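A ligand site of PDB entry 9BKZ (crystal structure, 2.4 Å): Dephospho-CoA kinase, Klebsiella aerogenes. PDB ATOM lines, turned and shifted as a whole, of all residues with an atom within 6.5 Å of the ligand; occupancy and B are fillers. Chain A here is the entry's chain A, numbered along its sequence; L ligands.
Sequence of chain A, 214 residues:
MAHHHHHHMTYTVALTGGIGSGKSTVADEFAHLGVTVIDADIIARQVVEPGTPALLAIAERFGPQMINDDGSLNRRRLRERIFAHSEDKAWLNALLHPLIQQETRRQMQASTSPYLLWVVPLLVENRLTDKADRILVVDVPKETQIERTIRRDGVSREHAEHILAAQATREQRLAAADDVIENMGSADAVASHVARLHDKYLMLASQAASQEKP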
ATOM      1  N   GLY A  17      25.854 -11.531 -10.776  1.00  0.00           N
ATOM      2  CA  GLY A  17      25.839 -10.418 -11.709  1.00  0.00           C
ATOM      3  C   GLY A  17      24.512  -9.699 -11.732  1.00  0.00           C
ATOM      4  O   GLY A  17      23.462 -10.315 -11.536  1.00  0.00           O
ATOM      5  N   GLY A  18      24.537  -8.395 -11.960  1.00  0.00           N
ATOM      6  CA  GLY A  18      23.320  -7.612 -11.945  1.00  0.00           C
ATOM      7  C   GLY A  18      22.366  -8.036 -13.055  1.00  0.00           C
ATOM      8  O   GLY A  18      22.707  -8.731 -14.001  1.00  0.00           O
ATOM      9  N   ILE A  19      21.110  -7.574 -12.910  1.00  0.00           N
ATOM     10  CA  ILE A  19      20.096  -7.882 -13.905  1.00  0.00           C
ATOM     11  C   ILE A  19      20.535  -7.354 -15.259  1.00  0.00           C
ATOM     12  O   ILE A  19      20.957  -6.204 -15.391  1.00  0.00           O
ATOM     13  CB  ILE A  19      18.734  -7.286 -13.482  1.00  0.00           C
ATOM     14  CG1 ILE A  19      17.762  -7.306 -14.669  1.00  0.00           C
ATOM     15  CG2 ILE A  19      18.910  -5.858 -12.967  1.00  0.00           C
ATOM     16  CD1 ILE A  19      16.305  -7.315 -14.265  1.00  0.00           C
ATOM     17  N   GLY A  20      20.419  -8.209 -16.278  1.00  0.00           N
ATOM     18  CA  GLY A  20      20.761  -7.829 -17.638  1.00  0.00           C
ATOM     19  C   GLY A  20      22.216  -7.959 -17.999  1.00  0.00           C
ATOM     20  O   GLY A  20      22.615  -7.492 -19.067  1.00  0.00           O
ATOM     21  N   SER A  21      23.028  -8.591 -17.154  1.00  0.00           N
ATOM     22  CA  SER A  21      24.448  -8.762 -17.428  1.00  0.00           C
ATOM     23  C   SER A  21      24.752 -10.021 -18.218  1.00  0.00           C
ATOM     24  O   SER A  21      25.887 -10.174 -18.689  1.00  0.00           O
ATOM     25  CB  SER A  21      25.239  -8.797 -16.110  1.00  0.00           C
ATOM     26  OG  SER A  21      24.772  -9.832 -15.254  1.00  0.00           O
ATOM     27  N   GLY A  22      23.779 -10.902 -18.399  1.00  0.00           N
ATOM     28  CA  GLY A  22      23.982 -12.122 -19.140  1.00  0.00           C
ATOM     29  C   GLY A  22      24.293 -13.350 -18.318  1.00  0.00           C
ATOM     30  O   GLY A  22      24.910 -14.283 -18.844  1.00  0.00           O
ATOM     31  N   LYS A  23      23.888 -13.380 -17.052  1.00  0.00           N
ATOM     32  CA  LYS A  23      24.131 -14.545 -16.211  1.00  0.00           C
ATOM     33  C   LYS A  23      23.635 -15.826 -16.886  1.00  0.00           C
ATOM     34  O   LYS A  23      24.348 -16.832 -16.935  1.00  0.00           O
ATOM     35  CB  LYS A  23      23.451 -14.371 -14.847  1.00  0.00           C
ATOM     36  CG  LYS A  23      24.088 -13.316 -13.956  1.00  0.00           C
ATOM     37  CD  LYS A  23      23.548 -13.386 -12.532  1.00  0.00           C
ATOM     38  CE  LYS A  23      22.051 -13.122 -12.481  1.00  0.00           C
ATOM     39  NZ  LYS A  23      21.666 -11.865 -13.184  1.00  0.00           N
ATOM     40  N   SER A  24      22.401 -15.788 -17.407  1.00  0.00           N
ATOM     41  CA  SER A  24      21.817 -16.998 -17.972  1.00  0.00           C
ATOM     42  C   SER A  24      22.582 -17.474 -19.202  1.00  0.00           C
ATOM     43  O   SER A  24      22.818 -18.670 -19.378  1.00  0.00           O
ATOM     44  CB  SER A  24      20.344 -16.758 -18.317  1.00  0.00           C
ATOM     45  OG  SER A  24      19.534 -16.848 -17.165  1.00  0.00           O
ATOM     46  N   THR A  25      22.974 -16.539 -20.080  1.00  0.00           N
ATOM     47  CA  THR A  25      23.725 -16.929 -21.272  1.00  0.00           C
ATOM     48  C   THR A  25      25.062 -17.550 -20.892  1.00  0.00           C
ATOM     49  O   THR A  25      25.482 -18.545 -21.498  1.00  0.00           O
ATOM     50  CB  THR A  25      23.928 -15.709 -22.169  1.00  0.00           C
ATOM     51  OG1 THR A  25      22.715 -14.951 -22.245  1.00  0.00           O
ATOM     52  CG2 THR A  25      24.333 -16.154 -23.574  1.00  0.00           C
ATOM     53  N   VAL A  26      25.748 -16.975 -19.908  1.00  0.00           N
ATOM     54  CA  VAL A  26      27.034 -17.514 -19.482  1.00  0.00           C
ATOM     55  C   VAL A  26      26.850 -18.870 -18.805  1.00  0.00           C
ATOM     56  O   VAL A  26      27.596 -19.811 -19.077  1.00  0.00           O
ATOM     57  CB  VAL A  26      27.749 -16.510 -18.548  1.00  0.00           C
ATOM     58  CG1 VAL A  26      28.962 -17.148 -17.905  1.00  0.00           C
ATOM     59  CG2 VAL A  26      28.138 -15.254 -19.315  1.00  0.00           C
ATOM     60  N   VAL A 138      29.694 -11.874 -13.627  1.00  0.00           N
ATOM     61  CA  VAL A 138      29.423 -11.431 -14.992  1.00  0.00           C
ATOM     62  C   VAL A 138      29.143  -9.940 -14.936  1.00  0.00           C
ATOM     63  O   VAL A 138      28.214  -9.495 -14.255  1.00  0.00           O
ATOM     64  CB  VAL A 138      28.239 -12.198 -15.601  1.00  0.00           C
ATOM     65  CG1 VAL A 138      27.918 -11.667 -16.991  1.00  0.00           C
ATOM     66  CG2 VAL A 138      28.547 -13.694 -15.658  1.00  0.00           C
ATOM     67  N   ARG A 148      19.519  -4.132 -22.093  1.00  0.00           N
ATOM     68  CA  ARG A 148      19.271  -5.568 -22.182  1.00  0.00           C
ATOM     69  C   ARG A 148      18.122  -6.010 -21.300  1.00  0.00           C
ATOM     70  O   ARG A 148      17.491  -7.035 -21.583  1.00  0.00           O
ATOM     71  CB  ARG A 148      20.547  -6.342 -21.816  1.00  0.00           C
ATOM     72  CG  ARG A 148      21.652  -6.204 -22.846  1.00  0.00           C
ATOM     73  CD  ARG A 148      22.862  -7.070 -22.510  1.00  0.00           C
ATOM     74  NE  ARG A 148      24.000  -6.777 -23.370  1.00  0.00           N
ATOM     75  CZ  ARG A 148      25.175  -7.377 -23.295  1.00  0.00           C
ATOM     76  NH1 ARG A 148      25.419  -8.326 -22.401  1.00  0.00           N
ATOM     77  NH2 ARG A 148      26.146  -7.014 -24.136  1.00  0.00           N
ATOM     78  N   THR A 149      17.818  -5.265 -20.243  1.00  0.00           N
ATOM     79  CA  THR A 149      16.627  -5.533 -19.454  1.00  0.00           C
ATOM     80  C   THR A 149      15.358  -5.187 -20.231  1.00  0.00           C
ATOM     81  O   THR A 149      14.374  -5.923 -20.185  1.00  0.00           O
ATOM     82  CB  THR A 149      16.667  -4.751 -18.141  1.00  0.00           C
ATOM     83  OG1 THR A 149      17.533  -5.407 -17.211  1.00  0.00           O
ATOM     84  CG2 THR A 149      15.272  -4.608 -17.540  1.00  0.00           C
ATOM     85  N   ARG A 151      14.726  -5.126 -23.506  1.00  0.00           N
ATOM     86  CA  ARG A 151      14.383  -6.009 -24.613  1.00  0.00           C
ATOM     87  C   ARG A 151      14.240  -7.465 -24.172  1.00  0.00           C
ATOM     88  O   ARG A 151      13.542  -8.244 -24.827  1.00  0.00           O
ATOM     89  CB  ARG A 151      15.425  -5.905 -25.726  1.00  0.00           C
ATOM     90  CG  ARG A 151      16.711  -6.700 -25.529  1.00  0.00           C
ATOM     91  CD  ARG A 151      17.531  -6.721 -26.831  1.00  0.00           C
ATOM     92  NE  ARG A 151      16.729  -7.173 -27.969  1.00  0.00           N
ATOM     93  CZ  ARG A 151      16.878  -8.336 -28.578  1.00  0.00           C
ATOM     94  NH1 ARG A 151      17.825  -9.188 -28.234  1.00  0.00           N
ATOM     95  NH2 ARG A 151      16.049  -8.654 -29.574  1.00  0.00           N
ATOM     96  N   ARG A 152      14.905  -7.866 -23.082  1.00  0.00           N
ATOM     97  CA  ARG A 152      14.754  -9.238 -22.609  1.00  0.00           C
ATOM     98  C   ARG A 152      13.429  -9.446 -21.892  1.00  0.00           C
ATOM     99  O   ARG A 152      12.695 -10.402 -22.164  1.00  0.00           O
ATOM    100  CB  ARG A 152      15.926  -9.610 -21.681  1.00  0.00           C
ATOM    101  CG  ARG A 152      15.796 -10.987 -21.031  1.00  0.00           C
ATOM    102  CD  ARG A 152      15.800 -12.106 -22.059  1.00  0.00           C
ATOM    103  NE  ARG A 152      15.350 -13.383 -21.503  1.00  0.00           N
ATOM    104  CZ  ARG A 152      16.155 -14.316 -21.025  1.00  0.00           C
ATOM    105  NH1 ARG A 152      17.472 -14.159 -20.989  1.00  0.00           N
ATOM    106  NH2 ARG A 152      15.621 -15.451 -20.553  1.00  0.00           N
ATOM    107  N   ASP A 153      13.095  -8.540 -20.971  1.00  0.00           N
ATOM    108  CA  ASP A 153      11.876  -8.671 -20.181  1.00  0.00           C
ATOM    109  C   ASP A 153      10.679  -7.943 -20.787  1.00  0.00           C
ATOM    110  O   ASP A 153       9.543  -8.262 -20.442  1.00  0.00           O
ATOM    111  CB  ASP A 153      12.112  -8.131 -18.766  1.00  0.00           C
ATOM    112  CG  ASP A 153      13.105  -8.968 -17.983  1.00  0.00           C
ATOM    113  OD1 ASP A 153      13.608  -9.984 -18.533  1.00  0.00           O
ATOM    114  OD2 ASP A 153      13.401  -8.623 -16.821  1.00  0.00           O
ATOM    115  N   ASN A 183      30.796  -9.535 -20.253  1.00  0.00           N
ATOM    116  CA  ASN A 183      29.900 -10.086 -21.265  1.00  0.00           C
ATOM    117  C   ASN A 183      29.603  -9.025 -22.335  1.00  0.00           C
ATOM    118  O   ASN A 183      28.475  -8.614 -22.564  1.00  0.00           O
ATOM    119  CB  ASN A 183      28.618 -10.590 -20.627  1.00  0.00           C
ATOM    120  CG  ASN A 183      27.732 -11.334 -21.601  1.00  0.00           C
ATOM    121  OD1 ASN A 183      28.223 -11.991 -22.522  1.00  0.00           O
ATOM    122  ND2 ASN A 183      26.424 -11.226 -21.417  1.00  0.00           N
ATOM    123  N   MET A 184      30.672  -8.589 -22.997  1.00  0.00           N
ATOM    124  CA  MET A 184      30.605  -7.574 -24.030  1.00  0.00           C
ATOM    125  C   MET A 184      31.424  -8.027 -25.226  1.00  0.00           C
ATOM    126  O   MET A 184      32.221  -8.959 -25.152  1.00  0.00           O
ATOM    127  CB  MET A 184      31.126  -6.224 -23.515  1.00  0.00           C
ATOM    128  CG  MET A 184      30.436  -5.729 -22.244  1.00  0.00           C
ATOM    129  SD  MET A 184      28.713  -5.271 -22.527  1.00  0.00           S
ATOM    130  CE  MET A 184      28.904  -3.953 -23.727  1.00  0.00           C
ATOM    131  N   GLY A 185      31.214  -7.349 -26.355  1.00  0.00           N
ATOM    132  CA  GLY A 185      31.955  -7.666 -27.557  1.00  0.00           C
ATOM    133  C   GLY A 185      31.399  -8.879 -28.278  1.00  0.00           C
ATOM    134  O   GLY A 185      30.200  -9.145 -28.275  1.00  0.00           O
ATOM    135  N   SER A 186      32.306  -9.622 -28.915  1.00  0.00           N
ATOM    136  CA  SER A 186      31.915 -10.795 -29.696  1.00  0.00           C
ATOM    137  C   SER A 186      31.558 -11.947 -28.779  1.00  0.00           C
ATOM    138  O   SER A 186      32.214 -12.188 -27.760  1.00  0.00           O
ATOM    139  CB  SER A 186      33.051 -11.196 -30.635  1.00  0.00           C
ATOM    140  OG  SER A 186      32.619 -12.185 -31.552  1.00  0.00           O
ATOM    141  N   ALA A 187      30.497 -12.670 -29.136  1.00  0.00           N
ATOM    142  CA  ALA A 187      30.095 -13.831 -28.346  1.00  0.00           C
ATOM    143  C   ALA A 187      31.185 -14.898 -28.353  1.00  0.00           C
ATOM    144  O   ALA A 187      31.463 -15.511 -27.313  1.00  0.00           O
ATOM    145  CB  ALA A 187      28.785 -14.411 -28.892  1.00  0.00           C
ATOM    146  N   VAL A 190      33.633 -14.214 -25.811  1.00  0.00           N
ATOM    147  CA  VAL A 190      33.026 -14.503 -24.517  1.00  0.00           C
ATOM    148  C   VAL A 190      33.026 -16.003 -24.266  1.00  0.00           C
ATOM    149  O   VAL A 190      33.449 -16.476 -23.198  1.00  0.00           O
ATOM    150  CB  VAL A 190      31.610 -13.927 -24.440  1.00  0.00           C
ATOM    151  CG1 VAL A 190      30.937 -14.315 -23.133  1.00  0.00           C
ATOM    152  CG2 VAL A 190      31.636 -12.405 -24.587  1.00  0.00           C
HETATM  153  P1  LIG L   1      20.619 -12.184 -16.500  1.00  0.00           P
HETATM  154  O1  LIG L   1      20.440 -13.678 -16.524  1.00  0.00           O
HETATM  155  O2  LIG L   1      19.347 -11.393 -16.329  1.00  0.00           O
HETATM  156  O3  LIG L   1      21.767 -11.713 -15.649  1.00  0.00           O
HETATM  157  P2  LIG L   1      20.386 -12.569 -19.247  1.00  0.00           P
HETATM  158  O4  LIG L   1      21.155 -13.840 -19.538  1.00  0.00           O
HETATM  159  O5  LIG L   1      18.911 -12.602 -18.970  1.00  0.00           O
HETATM  160  O6  LIG L   1      21.099 -11.833 -18.002  1.00  0.00           O
HETATM  161  O7  LIG L   1      20.691 -11.514 -20.435  1.00  0.00           O
HETATM  162  C1  LIG L   1      19.706 -10.588 -20.861  1.00  0.00           C
HETATM  163  C2  LIG L   1      19.767 -10.432 -22.363  1.00  0.00           C
HETATM  164  O8  LIG L   1      21.052  -9.990 -22.801  1.00  0.00           O
HETATM  165  C3  LIG L   1      19.478 -11.760 -23.081  1.00  0.00           C
HETATM  166  O9  LIG L   1      18.337 -11.632 -23.926  1.00  0.00           O
HETATM  167  C4  LIG L   1      20.713 -12.042 -23.949  1.00  0.00           C
HETATM  168  O10 LIG L   1      20.337 -12.522 -25.232  1.00  0.00           O
HETATM  169  C5  LIG L   1      21.429 -10.683 -24.009  1.00  0.00           C
HETATM  170  N1  LIG L   1      22.877 -10.812 -24.165  1.00  0.00           N
HETATM  171  C6  LIG L   1      23.714 -11.555 -23.428  1.00  0.00           C
HETATM  172  N2  LIG L   1      24.990 -11.426 -23.878  1.00  0.00           N
HETATM  173  C7  LIG L   1      24.979 -10.585 -24.933  1.00  0.00           C
HETATM  174  C8  LIG L   1      25.971 -10.008 -25.870  1.00  0.00           C
HETATM  175  N3  LIG L   1      27.281 -10.324 -25.781  1.00  0.00           N
HETATM  176  N4  LIG L   1      25.516  -9.168 -26.820  1.00  0.00           N
HETATM  177  C9  LIG L   1      24.215  -8.844 -26.944  1.00  0.00           C
HETATM  178  N5  LIG L   1      23.261  -9.322 -26.119  1.00  0.00           N
HETATM  179  C10 LIG L   1      23.576 -10.186 -25.116  1.00  0.00           C
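O4 of the ligand is in hydrogen-bond range of N of Thr 25.
N of Gly 20 is in hydrogen-bond range of O2 of the ligand (3.4 Å).
An oxygen (O5) of the ligand is in salt-bridge range of the guanidinium group (NH1) of Arg 152, 2.9 Å away.
An oxygen (O3) of the ligand lies within salt-bridge range of the side-chain amino group (NZ) of Lys 23 (2.5 Å).
N2 of the ligand lies within hydrogen-bond range of ND2 of Asn 183.
OG1 of Thr 25 sits at hydrogen-bond distance from O4 of the ligand (3.3 Å).
The backbone NH (N) of Ser 24 is in hydrogen-bond range of an oxygen (O1) of the ligand (3.0 Å).
O6 of the ligand lies within hydrogen-bond range of N of Gly 22.
OG of Ser 24 lies within hydrogen-bond range of O1 of the ligand (3.4 Å).
NH1 of Arg 148 sits close to N2 of the ligand (3.5 Å).
The backbone NH of Lys 23 lies within hydrogen-bond range of an oxygen (O3) of the ligand (3.0 Å).
The guanidinium group of Arg 148 sits at hydrogen-bond distance from the side-chain sulfur of Met 184 (3.5 Å).
O of Gly 18 is in hydrogen-bond range of OG of Ser 21.
O of Ser 21 sits at hydrogen-bond distance from ND2 of Asn 183.
The side-chain amino group (NZ) of Lys 23 lies within hydrogen-bond range of the backbone carbonyl oxygen (O) of Gly 18.
NZ of Lys 23 lies within hydrogen-bond range of O of Gly 17 (2.9 Å).
NH1 of Arg 148 sits at hydrogen-bond distance from O of Asn 183, at 3.1 Å.
Merely in contact with the ligand: Gly 18 and Ser 21.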
